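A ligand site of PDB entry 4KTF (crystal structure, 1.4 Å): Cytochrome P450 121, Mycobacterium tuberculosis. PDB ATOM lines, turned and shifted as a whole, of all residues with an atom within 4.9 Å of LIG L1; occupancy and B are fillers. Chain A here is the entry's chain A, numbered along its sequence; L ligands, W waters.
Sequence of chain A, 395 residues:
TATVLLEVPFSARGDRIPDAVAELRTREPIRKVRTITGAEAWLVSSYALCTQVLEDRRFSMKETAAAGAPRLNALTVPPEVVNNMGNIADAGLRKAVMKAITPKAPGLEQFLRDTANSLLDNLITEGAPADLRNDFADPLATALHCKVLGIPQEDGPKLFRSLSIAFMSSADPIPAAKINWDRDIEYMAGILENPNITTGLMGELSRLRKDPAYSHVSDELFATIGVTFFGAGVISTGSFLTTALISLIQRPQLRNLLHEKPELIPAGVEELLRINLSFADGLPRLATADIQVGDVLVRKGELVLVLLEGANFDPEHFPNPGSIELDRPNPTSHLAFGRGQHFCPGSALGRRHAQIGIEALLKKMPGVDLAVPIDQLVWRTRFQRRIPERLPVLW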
ATOM      1  N   LEU A  54     -20.375  37.438 -13.374  1.00  0.00           N
ATOM      2  CA  LEU A  54     -21.676  36.863 -13.306  1.00  0.00           C
ATOM      3  C   LEU A  54     -22.773  37.489 -14.206  1.00  0.00           C
ATOM      4  O   LEU A  54     -23.690  36.787 -14.610  1.00  0.00           O
ATOM      5  CB  LEU A  54     -22.197  36.688 -11.908  1.00  0.00           C
ATOM      6  CG  LEU A  54     -21.385  35.750 -10.982  1.00  0.00           C
ATOM      7  CD1 LEU A  54     -21.960  35.780  -9.628  1.00  0.00           C
ATOM      8  CD2 LEU A  54     -21.349  34.347 -11.513  1.00  0.00           C
ATOM      9  N   MET A  61     -21.686  29.331 -18.336  1.00  0.00           N
ATOM     10  CA  MET A  61     -21.845  28.120 -17.587  1.00  0.00           C
ATOM     11  C   MET A  61     -21.845  26.901 -18.469  1.00  0.00           C
ATOM     12  O   MET A  61     -21.074  25.937 -18.255  1.00  0.00           O
ATOM     13  CB  MET A  61     -23.126  28.135 -16.724  1.00  0.00           C
ATOM     14  CG  MET A  61     -23.465  26.804 -16.050  1.00  0.00           C
ATOM     15  SD  MET A  61     -25.017  26.843 -15.153  1.00  0.00           S
ATOM     16  CE  MET A  61     -24.579  27.835 -13.762  1.00  0.00           C
ATOM     17  N   VAL A  82     -25.404  20.313 -17.429  1.00  0.00           N
ATOM     18  CA  VAL A  82     -24.815  21.604 -17.015  1.00  0.00           C
ATOM     19  C   VAL A  82     -25.671  22.732 -17.509  1.00  0.00           C
ATOM     20  O   VAL A  82     -25.733  23.783 -16.830  1.00  0.00           O
ATOM     21  CB  VAL A  82     -23.305  21.609 -17.461  1.00  0.00           C
ATOM     22  CG1 VAL A  82     -22.705  22.991 -17.167  1.00  0.00           C
ATOM     23  CG2 VAL A  82     -22.515  20.426 -16.801  1.00  0.00           C
ATOM     24  N   ASN A  84     -28.916  22.742 -17.526  1.00  0.00           N
ATOM     25  CA  ASN A  84     -30.265  22.342 -17.074  1.00  0.00           C
ATOM     26  C   ASN A  84     -31.237  23.448 -17.141  1.00  0.00           C
ATOM     27  O   ASN A  84     -32.315  23.235 -17.689  1.00  0.00           O
ATOM     28  CB  ASN A  84     -30.108  21.798 -15.707  1.00  0.00           C
ATOM     29  CG  ASN A  84     -31.287  20.977 -15.166  1.00  0.00           C
ATOM     30  OD1 ASN A  84     -31.969  20.238 -15.902  1.00  0.00           O
ATOM     31  ND2 ASN A  84     -31.493  21.071 -13.827  1.00  0.00           N
ATOM     32  N   MET A  85     -30.900  24.658 -16.721  1.00  0.00           N
ATOM     33  CA  MET A  85     -31.895  25.720 -16.781  1.00  0.00           C
ATOM     34  C   MET A  85     -32.205  26.166 -18.198  1.00  0.00           C
ATOM     35  O   MET A  85     -33.357  26.516 -18.535  1.00  0.00           O
ATOM     36  CB  MET A  85     -31.537  26.883 -15.834  1.00  0.00           C
ATOM     37  CG  MET A  85     -31.897  26.608 -14.366  1.00  0.00           C
ATOM     38  SD  MET A  85     -33.590  26.263 -13.789  1.00  0.00           S
ATOM     39  CE  MET A  85     -34.502  27.331 -14.889  1.00  0.00           C
ATOM     40  N   ILE A 101     -41.730  25.487  -6.828  1.00  0.00           N
ATOM     41  CA  ILE A 101     -40.670  25.420  -5.772  1.00  0.00           C
ATOM     42  C   ILE A 101     -40.669  26.683  -4.893  1.00  0.00           C
ATOM     43  O   ILE A 101     -39.733  26.945  -4.151  1.00  0.00           O
ATOM     44  CB  ILE A 101     -39.279  25.101  -6.361  1.00  0.00           C
ATOM     45  CG1 ILE A 101     -38.785  26.218  -7.221  1.00  0.00           C
ATOM     46  CG2 ILE A 101     -39.280  23.744  -7.102  1.00  0.00           C
ATOM     47  CD1 ILE A 101     -37.339  26.049  -7.686  1.00  0.00           C
ATOM     48  N   HIS A 145     -38.027  18.755   0.534  1.00  0.00           N
ATOM     49  CA  HIS A 145     -37.928  18.466  -0.887  1.00  0.00           C
ATOM     50  C   HIS A 145     -38.831  17.311  -1.286  1.00  0.00           C
ATOM     51  O   HIS A 145     -39.315  17.400  -2.429  1.00  0.00           O
ATOM     52  CB  HIS A 145     -36.465  18.391  -1.350  1.00  0.00           C
ATOM     53  CG  HIS A 145     -35.816  19.747  -1.357  1.00  0.00           C
ATOM     54  ND1 HIS A 145     -35.332  20.360  -0.195  1.00  0.00           N
ATOM     55  CD2 HIS A 145     -35.616  20.680  -2.360  1.00  0.00           C
ATOM     56  CE1 HIS A 145     -34.880  21.573  -0.485  1.00  0.00           C
ATOM     57  NE2 HIS A 145     -35.042  21.799  -1.772  1.00  0.00           N
ATOM     58  N   PHE A 229     -33.348  18.968  -9.126  1.00  0.00           N
ATOM     59  CA  PHE A 229     -33.932  19.905  -8.171  1.00  0.00           C
ATOM     60  C   PHE A 229     -33.938  19.306  -6.763  1.00  0.00           C
ATOM     61  O   PHE A 229     -33.626  20.013  -5.811  1.00  0.00           O
ATOM     62  CB  PHE A 229     -35.321  20.479  -8.623  1.00  0.00           C
ATOM     63  CG  PHE A 229     -35.179  21.616  -9.538  1.00  0.00           C
ATOM     64  CD1 PHE A 229     -34.574  21.471 -10.788  1.00  0.00           C
ATOM     65  CD2 PHE A 229     -35.571  22.942  -9.196  1.00  0.00           C
ATOM     66  CE1 PHE A 229     -34.367  22.556 -11.598  1.00  0.00           C
ATOM     67  CE2 PHE A 229     -35.377  24.000 -10.074  1.00  0.00           C
ATOM     68  CZ  PHE A 229     -34.841  23.776 -11.257  1.00  0.00           C
ATOM     69  N   ALA A 232     -29.865  19.440  -5.805  1.00  0.00           N
ATOM     70  CA  ALA A 232     -29.389  20.756  -5.557  1.00  0.00           C
ATOM     71  C   ALA A 232     -30.070  21.423  -4.377  1.00  0.00           C
ATOM     72  O   ALA A 232     -29.408  22.018  -3.538  1.00  0.00           O
ATOM     73  CB  ALA A 232     -29.510  21.614  -6.757  1.00  0.00           C
ATOM     74  N   GLY A 233     -31.398  21.224  -4.265  1.00  0.00           N
ATOM     75  CA  GLY A 233     -32.084  21.867  -3.194  1.00  0.00           C
ATOM     76  C   GLY A 233     -31.683  21.233  -1.862  1.00  0.00           C
ATOM     77  O   GLY A 233     -31.478  21.938  -0.851  1.00  0.00           O
ATOM     78  N   SER A 236     -28.059  22.017  -0.848  1.00  0.00           N
ATOM     79  CA  SER A 236     -27.796  23.453  -0.633  1.00  0.00           C
ATOM     80  C   SER A 236     -28.479  23.944   0.660  1.00  0.00           C
ATOM     81  O   SER A 236     -27.835  24.636   1.476  1.00  0.00           O
ATOM     82  CB  SER A 236     -28.270  24.303  -1.773  1.00  0.00           C
ATOM     83  OG  SER A 236     -27.587  23.961  -2.993  1.00  0.00           O
ATOM     84  N   THR A 237     -29.734  23.554   0.903  1.00  0.00           N
ATOM     85  CA  THR A 237     -30.474  23.946   2.100  1.00  0.00           C
ATOM     86  C   THR A 237     -29.900  23.214   3.318  1.00  0.00           C
ATOM     87  O   THR A 237     -29.732  23.865   4.368  1.00  0.00           O
ATOM     88  CB  THR A 237     -31.964  23.720   1.977  1.00  0.00           C
ATOM     89  OG1 THR A 237     -32.263  22.375   1.711  1.00  0.00           O
ATOM     90  CG2 THR A 237     -32.556  24.617   0.884  1.00  0.00           C
ATOM     91  N   PHE A 240     -26.368  24.815   3.953  1.00  0.00           N
ATOM     92  CA  PHE A 240     -26.461  26.171   4.425  1.00  0.00           C
ATOM     93  C   PHE A 240     -27.005  26.240   5.842  1.00  0.00           C
ATOM     94  O   PHE A 240     -26.436  26.896   6.683  1.00  0.00           O
ATOM     95  CB  PHE A 240     -27.328  27.056   3.481  1.00  0.00           C
ATOM     96  CG  PHE A 240     -27.622  28.406   4.109  1.00  0.00           C
ATOM     97  CD1 PHE A 240     -26.578  29.255   4.422  1.00  0.00           C
ATOM     98  CD2 PHE A 240     -28.877  28.741   4.532  1.00  0.00           C
ATOM     99  CE1 PHE A 240     -26.821  30.481   5.090  1.00  0.00           C
ATOM    100  CE2 PHE A 240     -29.057  29.920   5.263  1.00  0.00           C
ATOM    101  CZ  PHE A 240     -28.062  30.798   5.522  1.00  0.00           C
ATOM    102  N   LEU A 273     -26.727  34.226   5.297  1.00  0.00           N
ATOM    103  CA  LEU A 273     -26.449  33.969   3.884  1.00  0.00           C
ATOM    104  C   LEU A 273     -25.260  34.727   3.417  1.00  0.00           C
ATOM    105  O   LEU A 273     -24.377  34.161   2.724  1.00  0.00           O
ATOM    106  CB  LEU A 273     -27.681  34.289   2.984  1.00  0.00           C
ATOM    107  CG  LEU A 273     -28.815  33.344   3.088  1.00  0.00           C
ATOM    108  CD1 LEU A 273     -30.160  33.938   2.617  1.00  0.00           C
ATOM    109  CD2 LEU A 273     -28.528  32.062   2.203  1.00  0.00           C
ATOM    110  N   PHE A 279     -20.341  27.173  -0.151  1.00  0.00           N
ATOM    111  CA  PHE A 279     -19.776  26.788  -1.471  1.00  0.00           C
ATOM    112  C   PHE A 279     -18.317  26.629  -1.360  1.00  0.00           C
ATOM    113  O   PHE A 279     -17.593  27.568  -1.059  1.00  0.00           O
ATOM    114  CB  PHE A 279     -20.175  27.808  -2.583  1.00  0.00           C
ATOM    115  CG  PHE A 279     -21.515  27.576  -3.198  1.00  0.00           C
ATOM    116  CD1 PHE A 279     -22.668  27.591  -2.489  1.00  0.00           C
ATOM    117  CD2 PHE A 279     -21.602  27.204  -4.543  1.00  0.00           C
ATOM    118  CE1 PHE A 279     -23.903  27.294  -3.087  1.00  0.00           C
ATOM    119  CE2 PHE A 279     -22.817  26.914  -5.104  1.00  0.00           C
ATOM    120  CZ  PHE A 279     -23.921  26.920  -4.423  1.00  0.00           C
ATOM    121  N   LEU A 283     -17.627  29.639  -8.379  1.00  0.00           N
ATOM    122  CA  LEU A 283     -18.544  29.225  -9.379  1.00  0.00           C
ATOM    123  C   LEU A 283     -17.772  29.246 -10.758  1.00  0.00           C
ATOM    124  O   LEU A 283     -17.192  30.291 -11.111  1.00  0.00           O
ATOM    125  CB  LEU A 283     -19.723  30.240  -9.497  1.00  0.00           C
ATOM    126  CG  LEU A 283     -20.564  30.434  -8.231  1.00  0.00           C
ATOM    127  CD1 LEU A 283     -21.723  31.350  -8.478  1.00  0.00           C
ATOM    128  CD2 LEU A 283     -21.123  29.117  -7.713  1.00  0.00           C
ATOM    129  N   ARG A 285     -17.013  29.360 -14.782  1.00  0.00           N
ATOM    130  CA  ARG A 285     -17.492  29.869 -16.083  1.00  0.00           C
ATOM    131  C   ARG A 285     -16.339  29.718 -17.089  1.00  0.00           C
ATOM    132  O   ARG A 285     -15.157  29.834 -16.745  1.00  0.00           O
ATOM    133  CB  ARG A 285     -17.802  31.393 -15.950  1.00  0.00           C
ATOM    134  CG  ARG A 285     -18.989  31.783 -15.074  1.00  0.00           C
ATOM    135  CD  ARG A 285     -20.244  31.289 -15.607  1.00  0.00           C
ATOM    136  NE  ARG A 285     -21.422  31.776 -14.810  1.00  0.00           N
ATOM    137  CZ  ARG A 285     -21.997  31.161 -13.793  1.00  0.00           C
ATOM    138  NH1 ARG A 285     -21.559  30.042 -13.272  1.00  0.00           N
ATOM    139  NH2 ARG A 285     -23.079  31.710 -13.229  1.00  0.00           N
ATOM    140  N   LEU A 308     -17.521  33.306  -4.137  1.00  0.00           N
ATOM    141  CA  LEU A 308     -18.663  34.023  -3.512  1.00  0.00           C
ATOM    142  C   LEU A 308     -18.238  34.730  -2.234  1.00  0.00           C
ATOM    143  O   LEU A 308     -18.717  35.881  -1.990  1.00  0.00           O
ATOM    144  CB  LEU A 308     -19.780  33.077  -3.279  1.00  0.00           C
ATOM    145  CG  LEU A 308     -20.340  32.419  -4.558  1.00  0.00           C
ATOM    146  CD1 LEU A 308     -21.516  31.532  -4.146  1.00  0.00           C
ATOM    147  CD2 LEU A 308     -20.723  33.467  -5.583  1.00  0.00           C
ATOM    148  N   LEU A 335     -24.042  37.834  -2.894  1.00  0.00           N
ATOM    149  CA  LEU A 335     -23.989  36.835  -3.950  1.00  0.00           C
ATOM    150  C   LEU A 335     -24.230  35.405  -3.509  1.00  0.00           C
ATOM    151  O   LEU A 335     -23.856  34.424  -4.213  1.00  0.00           O
ATOM    152  CB  LEU A 335     -22.732  36.939  -4.796  1.00  0.00           C
ATOM    153  CG  LEU A 335     -22.348  38.329  -5.298  1.00  0.00           C
ATOM    154  CD1 LEU A 335     -21.219  38.186  -6.342  1.00  0.00           C
ATOM    155  CD2 LEU A 335     -23.452  39.193  -5.775  1.00  0.00           C
ATOM    156  N   ALA A 336     -24.823  35.206  -2.372  1.00  0.00           N
ATOM    157  CA  ALA A 336     -25.051  33.765  -1.882  1.00  0.00           C
ATOM    158  C   ALA A 336     -25.866  32.933  -2.793  1.00  0.00           C
ATOM    159  O   ALA A 336     -25.670  31.693  -2.802  1.00  0.00           O
ATOM    160  CB  ALA A 336     -25.662  33.726  -0.508  1.00  0.00           C
ATOM    161  N   PHE A 337     -26.760  33.546  -3.584  1.00  0.00           N
ATOM    162  CA  PHE A 337     -27.590  32.819  -4.530  1.00  0.00           C
ATOM    163  C   PHE A 337     -27.043  33.112  -5.969  1.00  0.00           C
ATOM    164  O   PHE A 337     -27.805  32.826  -6.942  1.00  0.00           O
ATOM    165  CB  PHE A 337     -29.068  33.240  -4.410  1.00  0.00           C
ATOM    166  CG  PHE A 337     -29.690  32.842  -3.104  1.00  0.00           C
ATOM    167  CD1 PHE A 337     -29.836  31.483  -2.764  1.00  0.00           C
ATOM    168  CD2 PHE A 337     -30.184  33.790  -2.205  1.00  0.00           C
ATOM    169  CE1 PHE A 337     -30.492  31.155  -1.569  1.00  0.00           C
ATOM    170  CE2 PHE A 337     -30.773  33.416  -1.007  1.00  0.00           C
ATOM    171  CZ  PHE A 337     -31.023  32.107  -0.704  1.00  0.00           C
ATOM    172  N   GLY A 338     -25.864  33.613  -6.125  1.00  0.00           N
ATOM    173  CA  GLY A 338     -25.385  34.005  -7.447  1.00  0.00           C
ATOM    174  C   GLY A 338     -26.026  35.323  -7.896  1.00  0.00           C
ATOM    175  O   GLY A 338     -26.401  36.165  -7.051  1.00  0.00           O
ATOM    176  N   GLN A 341     -27.897  35.593 -15.095  1.00  0.00           N
ATOM    177  CA  GLN A 341     -28.669  34.562 -15.808  1.00  0.00           C
ATOM    178  C   GLN A 341     -28.971  33.332 -14.933  1.00  0.00           C
ATOM    179  O   GLN A 341     -30.055  32.732 -15.031  1.00  0.00           O
ATOM    180  CB  GLN A 341     -27.895  34.120 -17.059  1.00  0.00           C
ATOM    181  CG  GLN A 341     -28.542  33.051 -17.882  1.00  0.00           C
ATOM    182  CD  GLN A 341     -29.768  33.515 -18.640  1.00  0.00           C
ATOM    183  OE1 GLN A 341     -30.519  32.624 -19.172  1.00  0.00           O
ATOM    184  NE2 GLN A 341     -29.932  34.798 -18.831  1.00  0.00           N
ATOM    185  N   HIS A 342     -28.005  32.925 -14.115  1.00  0.00           N
ATOM    186  CA  HIS A 342     -28.096  31.705 -13.336  1.00  0.00           C
ATOM    187  C   HIS A 342     -28.388  31.819 -11.862  1.00  0.00           C
ATOM    188  O   HIS A 342     -28.197  30.919 -11.078  1.00  0.00           O
ATOM    189  CB  HIS A 342     -26.818  30.848 -13.569  1.00  0.00           C
ATOM    190  CG  HIS A 342     -26.653  30.454 -15.005  1.00  0.00           C
ATOM    191  ND1 HIS A 342     -27.436  29.495 -15.579  1.00  0.00           N
ATOM    192  CD2 HIS A 342     -25.760  30.854 -15.940  1.00  0.00           C
ATOM    193  CE1 HIS A 342     -27.101  29.366 -16.846  1.00  0.00           C
ATOM    194  NE2 HIS A 342     -26.101  30.181 -17.071  1.00  0.00           N
ATOM    195  N   PHE A 343     -28.926  32.999 -11.488  1.00  0.00           N
ATOM    196  CA  PHE A 343     -29.445  33.259 -10.157  1.00  0.00           C
ATOM    197  C   PHE A 343     -30.276  32.068  -9.693  1.00  0.00           C
ATOM    198  O   PHE A 343     -31.115  31.540 -10.415  1.00  0.00           O
ATOM    199  CB  PHE A 343     -30.282  34.546 -10.135  1.00  0.00           C
ATOM    200  CG  PHE A 343     -30.715  34.927  -8.755  1.00  0.00           C
ATOM    201  CD1 PHE A 343     -29.846  35.590  -7.945  1.00  0.00           C
ATOM    202  CD2 PHE A 343     -31.966  34.578  -8.302  1.00  0.00           C
ATOM    203  CE1 PHE A 343     -30.242  35.996  -6.644  1.00  0.00           C
ATOM    204  CE2 PHE A 343     -32.335  34.897  -6.960  1.00  0.00           C
ATOM    205  CZ  PHE A 343     -31.469  35.580  -6.170  1.00  0.00           C
ATOM    206  N   CYS A 344     -30.059  31.644  -8.465  1.00  0.00           N
ATOM    207  CA  CYS A 344     -30.657  30.419  -7.926  1.00  0.00           C
ATOM    208  C   CYS A 344     -32.213  30.423  -8.123  1.00  0.00           C
ATOM    209  O   CYS A 344     -32.851  31.332  -7.543  1.00  0.00           O
ATOM    210  CB  CYS A 344     -30.321  30.254  -6.449  1.00  0.00           C
ATOM    211  SG  CYS A 344     -31.066  28.819  -5.710  1.00  0.00           S
ATOM    212  N   PRO A 345     -32.811  29.422  -8.695  1.00  0.00           N
ATOM    213  CA  PRO A 345     -34.309  29.407  -8.809  1.00  0.00           C
ATOM    214  C   PRO A 345     -34.963  29.022  -7.530  1.00  0.00           C
ATOM    215  O   PRO A 345     -36.172  29.250  -7.352  1.00  0.00           O
ATOM    216  CB  PRO A 345     -34.551  28.337  -9.873  1.00  0.00           C
ATOM    217  CG  PRO A 345     -33.397  27.432  -9.717  1.00  0.00           C
ATOM    218  CD  PRO A 345     -32.216  28.307  -9.428  1.00  0.00           C
ATOM    219  N   GLY A 346     -34.239  28.553  -6.536  1.00  0.00           N
ATOM    220  CA  GLY A 346     -34.783  28.075  -5.258  1.00  0.00           C
ATOM    221  C   GLY A 346     -34.585  29.060  -4.081  1.00  0.00           C
ATOM    222  O   GLY A 346     -34.764  28.673  -2.951  1.00  0.00           O
ATOM    223  N   LEU A 349     -37.351  29.513  -1.321  1.00  0.00           N
ATOM    224  CA  LEU A 349     -37.459  28.287  -0.650  1.00  0.00           C
ATOM    225  C   LEU A 349     -36.265  28.104   0.340  1.00  0.00           C
ATOM    226  O   LEU A 349     -36.443  27.629   1.505  1.00  0.00           O
ATOM    227  CB  LEU A 349     -37.571  27.087  -1.575  1.00  0.00           C
ATOM    228  CG  LEU A 349     -37.962  25.798  -0.955  1.00  0.00           C
ATOM    229  CD1 LEU A 349     -39.331  25.727  -0.296  1.00  0.00           C
ATOM    230  CD2 LEU A 349     -37.851  24.692  -1.984  1.00  0.00           C
ATOM    231  N   GLY A 350     -35.024  28.361  -0.147  1.00  0.00           N
ATOM    232  CA  GLY A 350     -33.845  28.268   0.698  1.00  0.00           C
ATOM    233  C   GLY A 350     -33.972  29.202   1.902  1.00  0.00           C
ATOM    234  O   GLY A 350     -33.636  28.804   3.048  1.00  0.00           O
HETATM  235  C1  LIG L   1     -28.102  27.699  -8.697  1.00  0.00           C
HETATM  236  C2  LIG L   1     -27.029  28.735  -4.114  1.00  0.00           C
HETATM  237  C3  LIG L   1     -31.132  26.472  -2.735  1.00  0.00           C
HETATM  238  C4  LIG L   1     -31.615  24.823  -7.156  1.00  0.00           C
HETATM  239  C5  LIG L   1     -27.511  28.298  -7.542  1.00  0.00           C
HETATM  240  C6  LIG L   1     -26.385  29.190  -7.570  1.00  0.00           C
HETATM  241  C7  LIG L   1     -26.048  29.481  -6.253  1.00  0.00           C
HETATM  242  C8  LIG L   1     -26.969  28.724  -5.434  1.00  0.00           C
HETATM  243  C9  LIG L   1     -24.904  30.258  -5.759  1.00  0.00           C
HETATM  244  C10 LIG L   1     -25.751  29.777  -8.798  1.00  0.00           C
HETATM  245  C11 LIG L   1     -24.769  28.827  -9.484  1.00  0.00           C
HETATM  246  C12 LIG L   1     -23.998  29.478 -10.556  1.00  0.00           C
HETATM  247  O1  LIG L   1     -24.389  30.596 -11.065  1.00  0.00           O
HETATM  248  O2  LIG L   1     -22.966  28.892 -11.089  1.00  0.00           O
HETATM  249  C13 LIG L   1     -28.029  28.147  -3.293  1.00  0.00           C
HETATM  250  C14 LIG L   1     -28.159  28.316  -1.859  1.00  0.00           C
HETATM  251  C15 LIG L   1     -29.309  27.694  -1.498  1.00  0.00           C
HETATM  252  C16 LIG L   1     -29.912  27.127  -2.704  1.00  0.00           C
HETATM  253  C17 LIG L   1     -27.141  29.038  -1.037  1.00  0.00           C
HETATM  254  C18 LIG L   1     -29.918  27.514  -0.136  1.00  0.00           C
HETATM  255  C19 LIG L   1     -29.693  28.365   0.852  1.00  0.00           C
HETATM  256  C20 LIG L   1     -31.686  25.884  -3.826  1.00  0.00           C
HETATM  257  C21 LIG L   1     -32.933  25.178  -3.840  1.00  0.00           C
HETATM  258  C22 LIG L   1     -33.017  24.638  -5.073  1.00  0.00           C
HETATM  259  C23 LIG L   1     -31.914  25.095  -5.873  1.00  0.00           C
HETATM  260  C24 LIG L   1     -33.852  24.993  -2.710  1.00  0.00           C
HETATM  261  C25 LIG L   1     -34.108  23.831  -5.655  1.00  0.00           C
HETATM  262  C26 LIG L   1     -35.150  23.346  -5.137  1.00  0.00           C
HETATM  263  C27 LIG L   1     -30.616  25.337  -7.943  1.00  0.00           C
HETATM  264  C28 LIG L   1     -30.454  25.067  -9.396  1.00  0.00           C
HETATM  265  C29 LIG L   1     -29.479  25.910  -9.833  1.00  0.00           C
HETATM  266  C30 LIG L   1     -29.069  26.692  -8.638  1.00  0.00           C
HETATM  267  C31 LIG L   1     -31.246  24.073 -10.159  1.00  0.00           C
HETATM  268  C32 LIG L   1     -28.890  26.113 -11.182  1.00  0.00           C
HETATM  269  C33 LIG L   1     -29.508  27.331 -11.914  1.00  0.00           C
HETATM  270  C34 LIG L   1     -28.908  27.522 -13.305  1.00  0.00           C
HETATM  271  O3  LIG L   1     -29.243  28.604 -13.934  1.00  0.00           O
HETATM  272  O4  LIG L   1     -28.204  26.618 -13.846  1.00  0.00           O
HETATM  273  N1  LIG L   1     -27.907  28.063  -6.253  1.00  0.00           N
HETATM  274  N2  LIG L   1     -29.131  27.501  -3.679  1.00  0.00           N
HETATM  275  N3  LIG L   1     -31.095  25.913  -5.044  1.00  0.00           N
HETATM  276  N4  LIG L   1     -29.846  26.401  -7.556  1.00  0.00           N
HETATM  277 FE1  LIG L   1     -29.552  27.017  -5.672  1.00  0.00          FE
HETATM  278  C1  LG2 L   2     -26.014  20.171 -11.834  1.00  0.00           C
HETATM  279  C2  LG2 L   2     -26.988  20.983 -12.502  1.00  0.00           C
HETATM  280  C3  LG2 L   2     -28.106  21.398 -11.822  1.00  0.00           C
HETATM  281  O1  LG2 L   2     -29.014  22.266 -12.485  1.00  0.00           O
HETATM  282  C4  LG2 L   2     -28.350  20.949 -10.567  1.00  0.00           C
HETATM  283  C5  LG2 L   2     -27.347  20.116  -9.943  1.00  0.00           C
HETATM  284  C6  LG2 L   2     -26.175  19.739 -10.553  1.00  0.00           C
HETATM  285  C7  LG2 L   2     -25.154  18.919  -9.932  1.00  0.00           C
HETATM  286  C8  LG2 L   2     -23.821  19.365  -9.745  1.00  0.00           C
HETATM  287  N1  LG2 L   2     -23.295  20.652 -10.123  1.00  0.00           N
HETATM  288  N2  LG2 L   2     -23.041  18.444  -9.129  1.00  0.00           N
HETATM  289  N3  LG2 L   2     -23.922  17.442  -8.963  1.00  0.00           N
HETATM  290  C9  LG2 L   2     -25.164  17.646  -9.448  1.00  0.00           C
HETATM  291  C10 LG2 L   2     -26.106  16.582  -9.227  1.00  0.00           C
HETATM  292  C11 LG2 L   2     -25.718  15.265  -9.375  1.00  0.00           C
HETATM  293  C12 LG2 L   2     -26.534  14.209  -9.105  1.00  0.00           C
HETATM  294  C13 LG2 L   2     -27.819  14.432  -8.619  1.00  0.00           C
HETATM  295  O2  LG2 L   2     -28.534  13.348  -8.252  1.00  0.00           O
HETATM  296  C14 LG2 L   2     -28.306  15.772  -8.527  1.00  0.00           C
HETATM  297  C15 LG2 L   2     -27.444  16.789  -8.813  1.00  0.00           C
HETATM  298  O   HOH W   1     -22.026  26.415 -10.731  1.00  0.00           O
HETATM  299  O   HOH W   2     -27.967  24.046 -14.127  1.00  0.00           O
HETATM  300  O   HOH W   3     -28.150  25.162  -5.399  1.00  0.00           O
HETATM  301  O   HOH W   4     -31.276  29.978 -12.793  1.00  0.00           O
HETATM  302  O   HOH W   5     -25.453  33.095 -10.722  1.00  0.00           O
HETATM  303  O   HOH W   6     -28.307  26.021 -16.525  1.00  0.00           O
HETATM  304  O   HOH W   7     -30.932  30.167 -16.264  1.00  0.00           O
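The guanidinium group of Arg 285 lies within salt-bridge range of an oxygen (O1) of LIG L1 (2.8 Å). The side-chain amide nitrogen of Asn 84 is in hydrogen-bond range of an oxygen (O1) of LG2 L2. ND1 of His 342 lies within hydrogen-bond range of O3 of LIG L1 (2.6 Å). The side-chain sulfur (SG) of Cys 344 binds an iron atom (FE1) of LIG L1, 2.4 Å away.
Water W2 bridges O4 of LIG L1 and O1 of LG2 L2. Water W4 lies within hydrogen-bond range of an oxygen (O3) of LIG L1 and the backbone carbonyl oxygen of Phe 343. Water W6 lies within hydrogen-bond range of an oxygen (O4) of LIG L1 (2.7 Å), the backbone NH (N) of Met 85 (2.9 Å), the backbone carbonyl oxygen (O) of Val 82 (3.4 Å), the backbone NH (N) of Asn 84 (3.5 Å) and the side-chain sulfur (SD) of Met 61 (3.7 Å). Water W7 lies within hydrogen-bond range of O of Gln 341 (3.0 Å) and O3 of LIG L1 (3.3 Å).
OG of Ser 236 sits at hydrogen-bond distance from O of Ala 232. The backbone carbonyl oxygen (O) of Phe 337 is in hydrogen-bond range of the backbone NH (N) of Cys 344. The side-chain hydroxyl (OG1) of Thr 237 sits at hydrogen-bond distance from the backbone carbonyl oxygen (O) of Gly 233 (2.7 Å). ND1 of His 342 sits at hydrogen-bond distance from SD of Met 61. SG of Cys 344 lies close to N of Gly 346 (3.3 Å).
An oxygen (O4) of LIG L1 lies close to the side-chain sulfur of Met 61, at 3.5 Å. Met 85 touches LIG L1 (CG to C34, 3.3 Å). His 145 touches LIG L1 (NE2 to C24, 3.5 Å). Phe 229 touches LIG L1 (O to C26, 3.7 Å). Ala 232 touches LIG L1. Gly 233 touches LIG L1. CB of Ser 236 touches C16 of LIG L1 (3.4 Å). CG2 of Thr 237 touches C24 of LIG L1, 3.8 Å away. CB of Phe 240 touches C19 of LIG L1, 3.8 Å away. Phe 279 touches LIG L1. CD1 of Leu 283 touches C12 of LIG L1 (3.6 Å). CD1 of Leu 308 touches C9 of LIG L1 (3.96 Å). Ala 336 touches LIG L1. Phe 337 touches LIG L1. N of Gly 338 touches C9 of LIG L1, at 3.5 Å. Pro 345 touches LIG L1 (CD to N4, 3.6 Å). Gly 346 touches LIG L1. Hydrophobic or aromatic side chains within 4 Å of LIG L1: Met 61, Met 85, His 145, Phe 229, Ala 232, Phe 240, Phe 279, Leu 283, Leu 308, Phe 337, His 342 and Pro 345. Within 4 Å of LIG L1: Met 61, Met 85, His 145, Phe 229, Ala 232, Gly 233, Ser 236, Thr 237, Phe 240, Phe 279, Leu 283, Arg 285, Leu 308, Ala 336, Phe 337, Gly 338, His 342, Cys 344, Pro 345 and Gly 346.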
